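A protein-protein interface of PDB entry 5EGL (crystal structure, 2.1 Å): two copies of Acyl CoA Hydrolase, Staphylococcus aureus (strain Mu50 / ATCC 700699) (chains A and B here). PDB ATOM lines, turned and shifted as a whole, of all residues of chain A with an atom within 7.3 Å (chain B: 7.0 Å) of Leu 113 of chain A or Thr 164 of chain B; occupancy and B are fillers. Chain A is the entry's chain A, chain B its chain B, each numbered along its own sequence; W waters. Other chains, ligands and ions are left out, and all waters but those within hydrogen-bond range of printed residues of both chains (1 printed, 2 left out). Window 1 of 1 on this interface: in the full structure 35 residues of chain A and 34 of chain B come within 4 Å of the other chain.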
ATOM      1  N   LEU A  38      17.695  -0.120  -5.567  1.00  0.00           N
ATOM      2  CA  LEU A  38      17.544   0.702  -6.754  1.00  0.00           C
ATOM      3  C   LEU A  38      16.937  -0.160  -7.855  1.00  0.00           C
ATOM      4  O   LEU A  38      15.980   0.255  -8.510  1.00  0.00           O
ATOM      5  CB  LEU A  38      18.880   1.308  -7.190  1.00  0.00           C
ATOM      6  CG  LEU A  38      18.753   2.411  -8.242  1.00  0.00           C
ATOM      7  CD1 LEU A  38      18.145   3.664  -7.626  1.00  0.00           C
ATOM      8  CD2 LEU A  38      20.099   2.722  -8.873  1.00  0.00           C
ATOM      9  N   ILE A  42      13.408   0.526  -9.708  1.00  0.00           N
ATOM     10  CA  ILE A  42      13.427   0.633 -11.157  1.00  0.00           C
ATOM     11  C   ILE A  42      12.411  -0.331 -11.759  1.00  0.00           C
ATOM     12  O   ILE A  42      11.540   0.061 -12.554  1.00  0.00           O
ATOM     13  CB  ILE A  42      14.849   0.364 -11.712  1.00  0.00           C
ATOM     14  CG1 ILE A  42      15.761   1.537 -11.350  1.00  0.00           C
ATOM     15  CG2 ILE A  42      14.828   0.183 -13.239  1.00  0.00           C
ATOM     16  CD1 ILE A  42      17.249   1.299 -11.557  1.00  0.00           C
ATOM     17  N   SER A  65      20.247  -3.847 -18.531  1.00  0.00           N
ATOM     18  CA  SER A  65      21.391  -3.268 -17.859  1.00  0.00           C
ATOM     19  C   SER A  65      20.968  -2.176 -16.896  1.00  0.00           C
ATOM     20  O   SER A  65      19.926  -1.517 -17.061  1.00  0.00           O
ATOM     21  CB  SER A  65      22.410  -2.697 -18.850  1.00  0.00           C
ATOM     22  OG  SER A  65      21.926  -1.516 -19.456  1.00  0.00           O
ATOM     23  N   VAL A  66      21.820  -1.996 -15.898  1.00  0.00           N
ATOM     24  CA  VAL A  66      21.737  -0.875 -14.989  1.00  0.00           C
ATOM     25  C   VAL A  66      23.146  -0.308 -14.883  1.00  0.00           C
ATOM     26  O   VAL A  66      24.080  -1.006 -14.489  1.00  0.00           O
ATOM     27  CB  VAL A  66      21.233  -1.278 -13.591  1.00  0.00           C
ATOM     28  CG1 VAL A  66      21.173  -0.054 -12.675  1.00  0.00           C
ATOM     29  CG2 VAL A  66      19.878  -1.951 -13.665  1.00  0.00           C
ATOM     30  N   ASP A  67      23.303   0.956 -15.246  1.00  0.00           N
ATOM     31  CA  ASP A  67      24.587   1.609 -15.096  1.00  0.00           C
ATOM     32  C   ASP A  67      24.467   2.553 -13.905  1.00  0.00           C
ATOM     33  O   ASP A  67      23.648   3.483 -13.911  1.00  0.00           O
ATOM     34  CB  ASP A  67      24.967   2.350 -16.377  1.00  0.00           C
ATOM     35  CG  ASP A  67      26.449   2.627 -16.477  1.00  0.00           C
ATOM     36  OD1 ASP A  67      26.916   2.939 -17.594  1.00  0.00           O
ATOM     37  OD2 ASP A  67      27.149   2.530 -15.446  1.00  0.00           O
ATOM     38  N   PHE A  68      25.307   2.294 -12.900  1.00  0.00           N
ATOM     39  CA  PHE A  68      25.380   3.078 -11.666  1.00  0.00           C
ATOM     40  C   PHE A  68      26.433   4.152 -11.843  1.00  0.00           C
ATOM     41  O   PHE A  68      27.621   3.891 -11.714  1.00  0.00           O
ATOM     42  CB  PHE A  68      25.730   2.199 -10.455  1.00  0.00           C
ATOM     43  CG  PHE A  68      24.709   1.143 -10.138  1.00  0.00           C
ATOM     44  CD1 PHE A  68      24.834  -0.146 -10.631  1.00  0.00           C
ATOM     45  CD2 PHE A  68      23.609   1.448  -9.351  1.00  0.00           C
ATOM     46  CE1 PHE A  68      23.893  -1.111 -10.334  1.00  0.00           C
ATOM     47  CE2 PHE A  68      22.671   0.492  -9.048  1.00  0.00           C
ATOM     48  CZ  PHE A  68      22.801  -0.790  -9.546  1.00  0.00           C
ATOM     49  N   LEU A  69      25.984   5.348 -12.192  1.00  0.00           N
ATOM     50  CA  LEU A  69      26.882   6.417 -12.596  1.00  0.00           C
ATOM     51  C   LEU A  69      27.425   7.257 -11.443  1.00  0.00           C
ATOM     52  O   LEU A  69      28.619   7.546 -11.381  1.00  0.00           O
ATOM     53  CB  LEU A  69      26.151   7.319 -13.587  1.00  0.00           C
ATOM     54  CG  LEU A  69      25.539   6.561 -14.768  1.00  0.00           C
ATOM     55  CD1 LEU A  69      24.671   7.495 -15.605  1.00  0.00           C
ATOM     56  CD2 LEU A  69      26.610   5.903 -15.627  1.00  0.00           C
ATOM     57  N   VAL A  81      12.270   8.409 -13.881  1.00  0.00           N
ATOM     58  CA  VAL A  81      11.427   8.595 -15.057  1.00  0.00           C
ATOM     59  C   VAL A  81      11.496   7.355 -15.935  1.00  0.00           C
ATOM     60  O   VAL A  81      12.584   6.945 -16.360  1.00  0.00           O
ATOM     61  CB  VAL A  81      11.837   9.818 -15.884  1.00  0.00           C
ATOM     62  CG1 VAL A  81      10.795  10.088 -16.975  1.00  0.00           C
ATOM     63  CG2 VAL A  81      12.004  11.034 -14.995  1.00  0.00           C
ATOM     64  N   VAL A  95      12.878   2.209 -20.583  1.00  0.00           N
ATOM     65  CA  VAL A  95      14.068   2.893 -20.135  1.00  0.00           C
ATOM     66  C   VAL A  95      13.707   3.710 -18.903  1.00  0.00           C
ATOM     67  O   VAL A  95      12.667   4.389 -18.865  1.00  0.00           O
ATOM     68  CB  VAL A  95      14.686   3.798 -21.234  1.00  0.00           C
ATOM     69  CG1 VAL A  95      13.675   4.760 -21.795  1.00  0.00           C
ATOM     70  CG2 VAL A  95      15.905   4.556 -20.678  1.00  0.00           C
ATOM     71  N   VAL A  96      14.569   3.597 -17.895  1.00  0.00           N
ATOM     72  CA  VAL A  96      14.403   4.325 -16.655  1.00  0.00           C
ATOM     73  C   VAL A  96      15.627   5.181 -16.366  1.00  0.00           C
ATOM     74  O   VAL A  96      16.761   4.682 -16.292  1.00  0.00           O
ATOM     75  CB  VAL A  96      14.173   3.391 -15.453  1.00  0.00           C
ATOM     76  CG1 VAL A  96      13.866   4.232 -14.195  1.00  0.00           C
ATOM     77  CG2 VAL A  96      13.022   2.461 -15.724  1.00  0.00           C
ATOM     78  N   GLN A  97      15.363   6.472 -16.194  1.00  0.00           N
ATOM     79  CA  GLN A  97      16.365   7.435 -15.793  1.00  0.00           C
ATOM     80  C   GLN A  97      16.213   7.671 -14.309  1.00  0.00           C
ATOM     81  O   GLN A  97      15.085   7.891 -13.828  1.00  0.00           O
ATOM     82  CB  GLN A  97      16.192   8.762 -16.523  1.00  0.00           C
ATOM     83  CG  GLN A  97      16.187   8.689 -18.028  1.00  0.00           C
ATOM     84  CD  GLN A  97      15.634   9.958 -18.644  1.00  0.00           C
ATOM     85  OE1 GLN A  97      16.245  11.024 -18.559  1.00  0.00           O
ATOM     86  NE2 GLN A  97      14.456   9.855 -19.231  1.00  0.00           N
ATOM     87  N   ILE A  98      17.325   7.604 -13.583  1.00  0.00           N
ATOM     88  CA  ILE A  98      17.306   7.894 -12.157  1.00  0.00           C
ATOM     89  C   ILE A  98      18.204   9.093 -11.899  1.00  0.00           C
ATOM     90  O   ILE A  98      19.434   9.033 -12.108  1.00  0.00           O
ATOM     91  CB  ILE A  98      17.761   6.703 -11.299  1.00  0.00           C
ATOM     92  CG1 ILE A  98      16.939   5.459 -11.612  1.00  0.00           C
ATOM     93  CG2 ILE A  98      17.682   7.053  -9.817  1.00  0.00           C
ATOM     94  CD1 ILE A  98      17.419   4.663 -12.840  1.00  0.00           C
ATOM     95  N   LEU A 110      22.286  12.914 -13.204  1.00  0.00           N
ATOM     96  CA  LEU A 110      21.873  11.580 -13.595  1.00  0.00           C
ATOM     97  C   LEU A 110      22.687  10.586 -12.784  1.00  0.00           C
ATOM     98  O   LEU A 110      23.901  10.518 -12.912  1.00  0.00           O
ATOM     99  CB  LEU A 110      22.071  11.353 -15.095  1.00  0.00           C
ATOM    100  CG  LEU A 110      21.586   9.995 -15.607  1.00  0.00           C
ATOM    101  CD1 LEU A 110      20.074   9.911 -15.542  1.00  0.00           C
ATOM    102  CD2 LEU A 110      22.067   9.728 -17.015  1.00  0.00           C
ATOM    103  N   ALA A 111      22.020   9.871 -11.886  1.00  0.00           N
ATOM    104  CA  ALA A 111      22.692   8.921 -11.004  1.00  0.00           C
ATOM    105  C   ALA A 111      22.746   7.537 -11.603  1.00  0.00           C
ATOM    106  O   ALA A 111      23.677   6.777 -11.329  1.00  0.00           O
ATOM    107  CB  ALA A 111      22.006   8.863  -9.665  1.00  0.00           C
ATOM    108  N   ALA A 112      21.702   7.164 -12.335  1.00  0.00           N
ATOM    109  CA  ALA A 112      21.686   5.831 -12.928  1.00  0.00           C
ATOM    110  C   ALA A 112      20.836   5.742 -14.172  1.00  0.00           C
ATOM    111  O   ALA A 112      19.887   6.510 -14.366  1.00  0.00           O
ATOM    112  CB  ALA A 112      21.197   4.797 -11.909  1.00  0.00           C
ATOM    113  N   LEU A 113      21.186   4.778 -15.012  1.00  0.00           N
ATOM    114  CA  LEU A 113      20.438   4.571 -16.242  1.00  0.00           C
ATOM    115  C   LEU A 113      20.126   3.097 -16.384  1.00  0.00           C
ATOM    116  O   LEU A 113      20.999   2.258 -16.181  1.00  0.00           O
ATOM    117  CB  LEU A 113      21.228   5.085 -17.434  1.00  0.00           C
ATOM    118  CG  LEU A 113      20.531   5.199 -18.776  1.00  0.00           C
ATOM    119  CD1 LEU A 113      19.328   6.131 -18.691  1.00  0.00           C
ATOM    120  CD2 LEU A 113      21.536   5.731 -19.778  1.00  0.00           C
ATOM    121  N   SER A 114      18.882   2.770 -16.701  1.00  0.00           N
ATOM    122  CA  SER A 114      18.522   1.368 -16.803  1.00  0.00           C
ATOM    123  C   SER A 114      17.613   1.051 -17.977  1.00  0.00           C
ATOM    124  O   SER A 114      16.782   1.867 -18.377  1.00  0.00           O
ATOM    125  CB  SER A 114      17.845   0.915 -15.510  1.00  0.00           C
ATOM    126  OG  SER A 114      17.391  -0.423 -15.626  1.00  0.00           O
ATOM    127  N   TYR A 115      17.797  -0.147 -18.524  1.00  0.00           N
ATOM    128  CA  TYR A 115      16.950  -0.640 -19.603  1.00  0.00           C
ATOM    129  C   TYR A 115      16.408  -2.010 -19.220  1.00  0.00           C
ATOM    130  O   TYR A 115      17.179  -2.874 -18.819  1.00  0.00           O
ATOM    131  CB  TYR A 115      17.735  -0.731 -20.920  1.00  0.00           C
ATOM    132  CG  TYR A 115      18.342   0.577 -21.353  1.00  0.00           C
ATOM    133  CD1 TYR A 115      19.628   0.931 -20.978  1.00  0.00           C
ATOM    134  CD2 TYR A 115      17.618   1.467 -22.125  1.00  0.00           C
ATOM    135  CE1 TYR A 115      20.176   2.137 -21.371  1.00  0.00           C
ATOM    136  CE2 TYR A 115      18.158   2.671 -22.520  1.00  0.00           C
ATOM    137  CZ  TYR A 115      19.435   3.000 -22.140  1.00  0.00           C
ATOM    138  OH  TYR A 115      19.971   4.201 -22.534  1.00  0.00           O
ATOM    139  N   LEU A 116      15.101  -2.207 -19.375  1.00  0.00           N
ATOM    140  CA  LEU A 116      14.472  -3.483 -19.045  1.00  0.00           C
ATOM    141  C   LEU A 116      13.534  -3.949 -20.146  1.00  0.00           C
ATOM    142  O   LEU A 116      13.011  -3.142 -20.906  1.00  0.00           O
ATOM    143  CB  LEU A 116      13.681  -3.386 -17.729  1.00  0.00           C
ATOM    144  CG  LEU A 116      14.401  -2.836 -16.494  1.00  0.00           C
ATOM    145  CD1 LEU A 116      14.351  -1.317 -16.492  1.00  0.00           C
ATOM    146  CD2 LEU A 116      13.799  -3.385 -15.208  1.00  0.00           C
ATOM    147  N   TRP A 142      15.388  10.565 -28.613  1.00  0.00           N
ATOM    148  CA  TRP A 142      16.715  10.010 -28.397  1.00  0.00           C
ATOM    149  C   TRP A 142      16.645   8.534 -28.002  1.00  0.00           C
ATOM    150  O   TRP A 142      17.287   7.671 -28.638  1.00  0.00           O
ATOM    151  CB  TRP A 142      17.470  10.790 -27.321  1.00  0.00           C
ATOM    152  CG  TRP A 142      18.809  10.195 -27.068  1.00  0.00           C
ATOM    153  CD1 TRP A 142      19.133   9.276 -26.110  1.00  0.00           C
ATOM    154  CD2 TRP A 142      20.009  10.446 -27.803  1.00  0.00           C
ATOM    155  NE1 TRP A 142      20.464   8.943 -26.205  1.00  0.00           N
ATOM    156  CE2 TRP A 142      21.024   9.655 -27.236  1.00  0.00           C
ATOM    157  CE3 TRP A 142      20.326  11.272 -28.882  1.00  0.00           C
ATOM    158  CZ2 TRP A 142      22.327   9.661 -27.710  1.00  0.00           C
ATOM    159  CZ3 TRP A 142      21.629  11.282 -29.352  1.00  0.00           C
ATOM    160  CH2 TRP A 142      22.611  10.479 -28.767  1.00  0.00           C
ATOM    161  N   PHE A 143      15.861   8.234 -26.965  1.00  0.00           N
ATOM    162  CA  PHE A 143      15.758   6.841 -26.515  1.00  0.00           C
ATOM    163  C   PHE A 143      15.108   5.934 -27.561  1.00  0.00           C
ATOM    164  O   PHE A 143      15.501   4.778 -27.732  1.00  0.00           O
ATOM    165  CB  PHE A 143      15.006   6.764 -25.182  1.00  0.00           C
ATOM    166  CG  PHE A 143      15.829   7.224 -24.011  1.00  0.00           C
ATOM    167  CD1 PHE A 143      16.990   6.556 -23.665  1.00  0.00           C
ATOM    168  CD2 PHE A 143      15.470   8.341 -23.287  1.00  0.00           C
ATOM    169  CE1 PHE A 143      17.756   6.981 -22.604  1.00  0.00           C
ATOM    170  CE2 PHE A 143      16.241   8.764 -22.222  1.00  0.00           C
ATOM    171  CZ  PHE A 143      17.378   8.088 -21.887  1.00  0.00           C
ATOM    172  N   THR A 146      17.757   5.324 -30.368  1.00  0.00           N
ATOM    173  CA  THR A 146      18.843   4.418 -30.004  1.00  0.00           C
ATOM    174  C   THR A 146      18.386   3.003 -29.596  1.00  0.00           C
ATOM    175  O   THR A 146      19.217   2.141 -29.318  1.00  0.00           O
ATOM    176  CB  THR A 146      19.679   5.024 -28.874  1.00  0.00           C
ATOM    177  OG1 THR A 146      18.824   5.365 -27.778  1.00  0.00           O
ATOM    178  CG2 THR A 146      20.387   6.272 -29.373  1.00  0.00           C
ATOM    179  N   ARG A 150      20.081  -1.415 -28.998  1.00  0.00           N
ATOM    180  CA  ARG A 150      19.991  -2.115 -27.717  1.00  0.00           C
ATOM    181  C   ARG A 150      19.244  -3.444 -27.879  1.00  0.00           C
ATOM    182  O   ARG A 150      19.628  -4.480 -27.326  1.00  0.00           O
ATOM    183  CB  ARG A 150      19.299  -1.241 -26.677  1.00  0.00           C
ATOM    184  CG  ARG A 150      20.165  -0.097 -26.185  1.00  0.00           C
ATOM    185  CD  ARG A 150      19.534   0.580 -24.996  1.00  0.00           C
ATOM    186  NE  ARG A 150      18.214   1.116 -25.307  1.00  0.00           N
ATOM    187  CZ  ARG A 150      17.987   2.329 -25.800  1.00  0.00           C
ATOM    188  NH1 ARG A 150      18.994   3.152 -26.061  1.00  0.00           N
ATOM    189  NH2 ARG A 150      16.746   2.719 -26.043  1.00  0.00           N
ATOM    190  N   ILE B 159      30.492   2.437 -23.808  1.00  0.00           N
ATOM    191  CA  ILE B 159      30.844   3.427 -24.820  1.00  0.00           C
ATOM    192  C   ILE B 159      29.582   4.089 -25.349  1.00  0.00           C
ATOM    193  O   ILE B 159      29.482   5.325 -25.338  1.00  0.00           O
ATOM    194  CB  ILE B 159      31.671   2.788 -25.958  1.00  0.00           C
ATOM    195  CG1 ILE B 159      33.057   2.432 -25.424  1.00  0.00           C
ATOM    196  CG2 ILE B 159      31.867   3.753 -27.096  1.00  0.00           C
ATOM    197  CD1 ILE B 159      33.848   1.483 -26.296  1.00  0.00           C
ATOM    198  N   GLU B 160      28.605   3.295 -25.777  1.00  0.00           N
ATOM    199  CA  GLU B 160      27.351   3.907 -26.235  1.00  0.00           C
ATOM    200  C   GLU B 160      26.633   4.718 -25.161  1.00  0.00           C
ATOM    201  O   GLU B 160      26.064   5.763 -25.457  1.00  0.00           O
ATOM    202  CB  GLU B 160      26.392   2.853 -26.786  1.00  0.00           C
ATOM    203  CG  GLU B 160      26.891   2.264 -28.067  1.00  0.00           C
ATOM    204  CD  GLU B 160      27.158   3.319 -29.119  1.00  0.00           C
ATOM    205  OE1 GLU B 160      26.392   4.306 -29.176  1.00  0.00           O
ATOM    206  OE2 GLU B 160      28.161   3.176 -29.850  1.00  0.00           O
ATOM    207  N   SER B 161      26.637   4.239 -23.923  1.00  0.00           N
ATOM    208  CA  SER B 161      25.962   4.941 -22.829  1.00  0.00           C
ATOM    209  C   SER B 161      26.484   6.363 -22.616  1.00  0.00           C
ATOM    210  O   SER B 161      25.712   7.278 -22.296  1.00  0.00           O
ATOM    211  CB  SER B 161      26.085   4.146 -21.525  1.00  0.00           C
ATOM    212  OG  SER B 161      27.347   4.342 -20.918  1.00  0.00           O
ATOM    213  N   LYS B 162      27.795   6.549 -22.737  1.00  0.00           N
ATOM    214  CA  LYS B 162      28.361   7.897 -22.584  1.00  0.00           C
ATOM    215  C   LYS B 162      27.719   8.944 -23.537  1.00  0.00           C
ATOM    216  O   LYS B 162      27.530  10.118 -23.170  1.00  0.00           O
ATOM    217  CB  LYS B 162      29.872   7.832 -22.778  1.00  0.00           C
ATOM    218  CG  LYS B 162      30.553   7.092 -21.641  1.00  0.00           C
ATOM    219  CD  LYS B 162      30.540   7.881 -20.349  1.00  0.00           C
ATOM    220  CE  LYS B 162      31.068   7.062 -19.188  1.00  0.00           C
ATOM    221  NZ  LYS B 162      30.020   6.151 -18.662  1.00  0.00           N
ATOM    222  N   GLN B 163      27.423   8.524 -24.756  1.00  0.00           N
ATOM    223  CA  GLN B 163      26.716   9.350 -25.736  1.00  0.00           C
ATOM    224  C   GLN B 163      25.331   9.790 -25.177  1.00  0.00           C
ATOM    225  O   GLN B 163      24.945  10.975 -25.243  1.00  0.00           O
ATOM    226  CB  GLN B 163      26.621   8.549 -27.045  1.00  0.00           C
ATOM    227  CG  GLN B 163      25.639   9.005 -28.115  1.00  0.00           C
ATOM    228  CD  GLN B 163      25.962   8.413 -29.491  1.00  0.00           C
ATOM    229  OE1 GLN B 163      27.104   8.042 -29.756  1.00  0.00           O
ATOM    230  NE2 GLN B 163      24.953   8.319 -30.363  1.00  0.00           N
ATOM    231  N   THR B 164      24.595   8.841 -24.608  1.00  0.00           N
ATOM    232  CA  THR B 164      23.283   9.148 -24.025  1.00  0.00           C
ATOM    233  C   THR B 164      23.395  10.072 -22.827  1.00  0.00           C
ATOM    234  O   THR B 164      22.645  11.043 -22.711  1.00  0.00           O
ATOM    235  CB  THR B 164      22.542   7.866 -23.614  1.00  0.00           C
ATOM    236  OG1 THR B 164      22.203   7.141 -24.795  1.00  0.00           O
ATOM    237  CG2 THR B 164      21.242   8.175 -22.893  1.00  0.00           C
ATOM    238  N   ILE B 165      24.348   9.796 -21.950  1.00  0.00           N
ATOM    239  CA  ILE B 165      24.557  10.652 -20.787  1.00  0.00           C
ATOM    240  C   ILE B 165      24.848  12.086 -21.221  1.00  0.00           C
ATOM    241  O   ILE B 165      24.292  13.040 -20.652  1.00  0.00           O
ATOM    242  CB  ILE B 165      25.696  10.107 -19.902  1.00  0.00           C
ATOM    243  CG1 ILE B 165      25.268   8.770 -19.300  1.00  0.00           C
ATOM    244  CG2 ILE B 165      26.045  11.075 -18.792  1.00  0.00           C
ATOM    245  CD1 ILE B 165      26.399   7.963 -18.691  1.00  0.00           C
ATOM    246  N   GLU B 166      25.736  12.268 -22.195  1.00  0.00           N
ATOM    247  CA  GLU B 166      25.988  13.627 -22.674  1.00  0.00           C
ATOM    248  C   GLU B 166      24.735  14.265 -23.262  1.00  0.00           C
ATOM    249  O   GLU B 166      24.441  15.438 -23.000  1.00  0.00           O
ATOM    250  CB  GLU B 166      27.125  13.646 -23.693  1.00  0.00           C
ATOM    251  CG  GLU B 166      27.389  15.029 -24.283  1.00  0.00           C
ATOM    252  CD  GLU B 166      27.810  16.063 -23.261  1.00  0.00           C
ATOM    253  OE1 GLU B 166      28.096  15.702 -22.101  1.00  0.00           O
ATOM    254  OE2 GLU B 166      27.804  17.258 -23.620  1.00  0.00           O
ATOM    255  N   TYR B 167      23.985  13.514 -24.058  1.00  0.00           N
ATOM    256  CA  TYR B 167      22.758  14.086 -24.596  1.00  0.00           C
ATOM    257  C   TYR B 167      21.813  14.530 -23.468  1.00  0.00           C
ATOM    258  O   TYR B 167      21.244  15.628 -23.508  1.00  0.00           O
ATOM    259  CB  TYR B 167      22.050  13.088 -25.505  1.00  0.00           C
ATOM    260  CG  TYR B 167      20.805  13.665 -26.124  1.00  0.00           C
ATOM    261  CD1 TYR B 167      20.869  14.382 -27.307  1.00  0.00           C
ATOM    262  CD2 TYR B 167      19.568  13.518 -25.513  1.00  0.00           C
ATOM    263  CE1 TYR B 167      19.734  14.928 -27.871  1.00  0.00           C
ATOM    264  CE2 TYR B 167      18.434  14.061 -26.069  1.00  0.00           C
ATOM    265  CZ  TYR B 167      18.522  14.762 -27.247  1.00  0.00           C
ATOM    266  OH  TYR B 167      17.388  15.300 -27.801  1.00  0.00           O
ATOM    267  N   LEU B 168      21.651  13.681 -22.458  1.00  0.00           N
ATOM    268  CA  LEU B 168      20.747  13.991 -21.363  1.00  0.00           C
ATOM    269  C   LEU B 168      21.260  15.184 -20.557  1.00  0.00           C
ATOM    270  O   LEU B 168      20.477  15.993 -20.064  1.00  0.00           O
ATOM    271  CB  LEU B 168      20.599  12.778 -20.448  1.00  0.00           C
ATOM    272  CG  LEU B 168      19.799  11.606 -21.010  1.00  0.00           C
ATOM    273  CD1 LEU B 168      19.749  10.506 -19.992  1.00  0.00           C
ATOM    274  CD2 LEU B 168      18.389  12.006 -21.440  1.00  0.00           C
ATOM    275  N   ALA B 169      22.578  15.316 -20.447  1.00  0.00           N
ATOM    276  CA  ALA B 169      23.144  16.477 -19.767  1.00  0.00           C
ATOM    277  C   ALA B 169      22.893  17.750 -20.566  1.00  0.00           C
ATOM    278  O   ALA B 169      22.642  18.811 -19.993  1.00  0.00           O
ATOM    279  CB  ALA B 169      24.625  16.292 -19.532  1.00  0.00           C
ATOM    280  N   GLN B 170      22.962  17.655 -21.886  1.00  0.00           N
ATOM    281  CA  GLN B 170      22.622  18.807 -22.712  1.00  0.00           C
ATOM    282  C   GLN B 170      21.134  19.149 -22.620  1.00  0.00           C
ATOM    283  O   GLN B 170      20.767  20.320 -22.601  1.00  0.00           O
ATOM    284  CB  GLN B 170      23.016  18.559 -24.166  1.00  0.00           C
ATOM    285  CG  GLN B 170      24.528  18.476 -24.370  1.00  0.00           C
ATOM    286  CD  GLN B 170      24.914  18.180 -25.804  1.00  0.00           C
ATOM    287  OE1 GLN B 170      24.069  18.144 -26.695  1.00  0.00           O
ATOM    288  NE2 GLN B 170      26.199  17.958 -26.032  1.00  0.00           N
HETATM  289  O   HOH W   1      29.669   4.181 -16.227  1.00  0.00           O
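Water W1 bridges the side-chain carboxylate of Asp 67 of chain A (3.1 Å) and the side-chain amino group of Lys 162 of chain B (3.2 Å).
Of the 12 printed residues of chain B, 6 touch a printed residue of chain A.
Hydrophobic or aromatic side chains of chain B that line the printed part of chain A: Ile 165, Tyr 167 and Leu 168.
Of the 23 printed residues of chain A, 7 touch a printed residue of chain B.
Among the printed residues, 10 pairs touch across the chains.
Among the printed residues, no Asp or Glu carboxylate lies within 4 Å of a Lys or Arg side-chain nitrogen of the other chain.
Among the printed residues, pairs that only touch across the chains: Asp 67 of chain A with Ser 161 of chain B (3.6 Å), Leu 69 of chain A with Ile 165 of chain B (3.6 Å), Gln 97 of chain A with Leu 168 of chain B (3.7 Å), Leu 110 of chain A with Leu 168 of chain B (3.9 Å), Leu 113 of chain A with Thr 164 of chain B (3.97 Å), Trp 142 of chain A with Gln 163 of chain B (3.4 Å), Trp 142 of chain A with Tyr 167 of chain B (3.5 Å), Phe 143 of chain A with Thr 164 of chain B (3.7 Å) and Phe 143 of chain A with Leu 168 of chain B (3.9 Å).
The indole nitrogen of Trp 142 of chain A is in hydrogen-bond range of the side-chain hydroxyl of Thr 164 of chain B (2.9 Å).
The backbone carbonyl oxygen of Ala 111 of chain A sits at hydrogen-bond distance from the backbone NH of Leu 69 of chain A, 2.8 Å away.
The backbone carbonyl oxygen of Trp 142 of chain A sits at hydrogen-bond distance from the side-chain hydroxyl of Thr 146 of chain A, 2.9 Å away.
The backbone carbonyl oxygen (O) of Phe 143 of chain A lies within hydrogen-bond range of the side-chain hydroxyl (OG1) of Thr 146 of chain A (3.4 Å).
O of Phe 143 of chain A sits at hydrogen-bond distance from NH2 of Arg 150 of chain A (2.9 Å).
O of Val 81 of chain A is in hydrogen-bond range of N of Gln 97 of chain A (2.8 Å).
N of Asp 67 of chain A sits at hydrogen-bond distance from O of Leu 113 of chain A (2.8 Å).
Leu 113 of chain A touches just one residue of chain B: Thr 164 (3.97 Å).
Thr 164 of chain B touches just these residues of chain A: Leu 113 (3.97 Å), Trp 142 (2.9 Å) and Phe 143 (3.7 Å).
Of the printed residues of chain B, Leu 69 of chain A touches Ile 165.
Printed residues of chain B within 4 Å of Gln 97 of chain A: Leu 168.
The nearest residue of chain B that does not touch Leu 113 of chain A is Leu 168 of chain B (4.6 Å).
The nearest printed residue of chain A that does not touch Tyr 167 of chain B is Phe 143 of chain A (6.4 Å).
No position is printed for both chains.
Of the 10 pairs that touch across the chains among the printed residues, none has its exchanged pair printed and touching as well.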
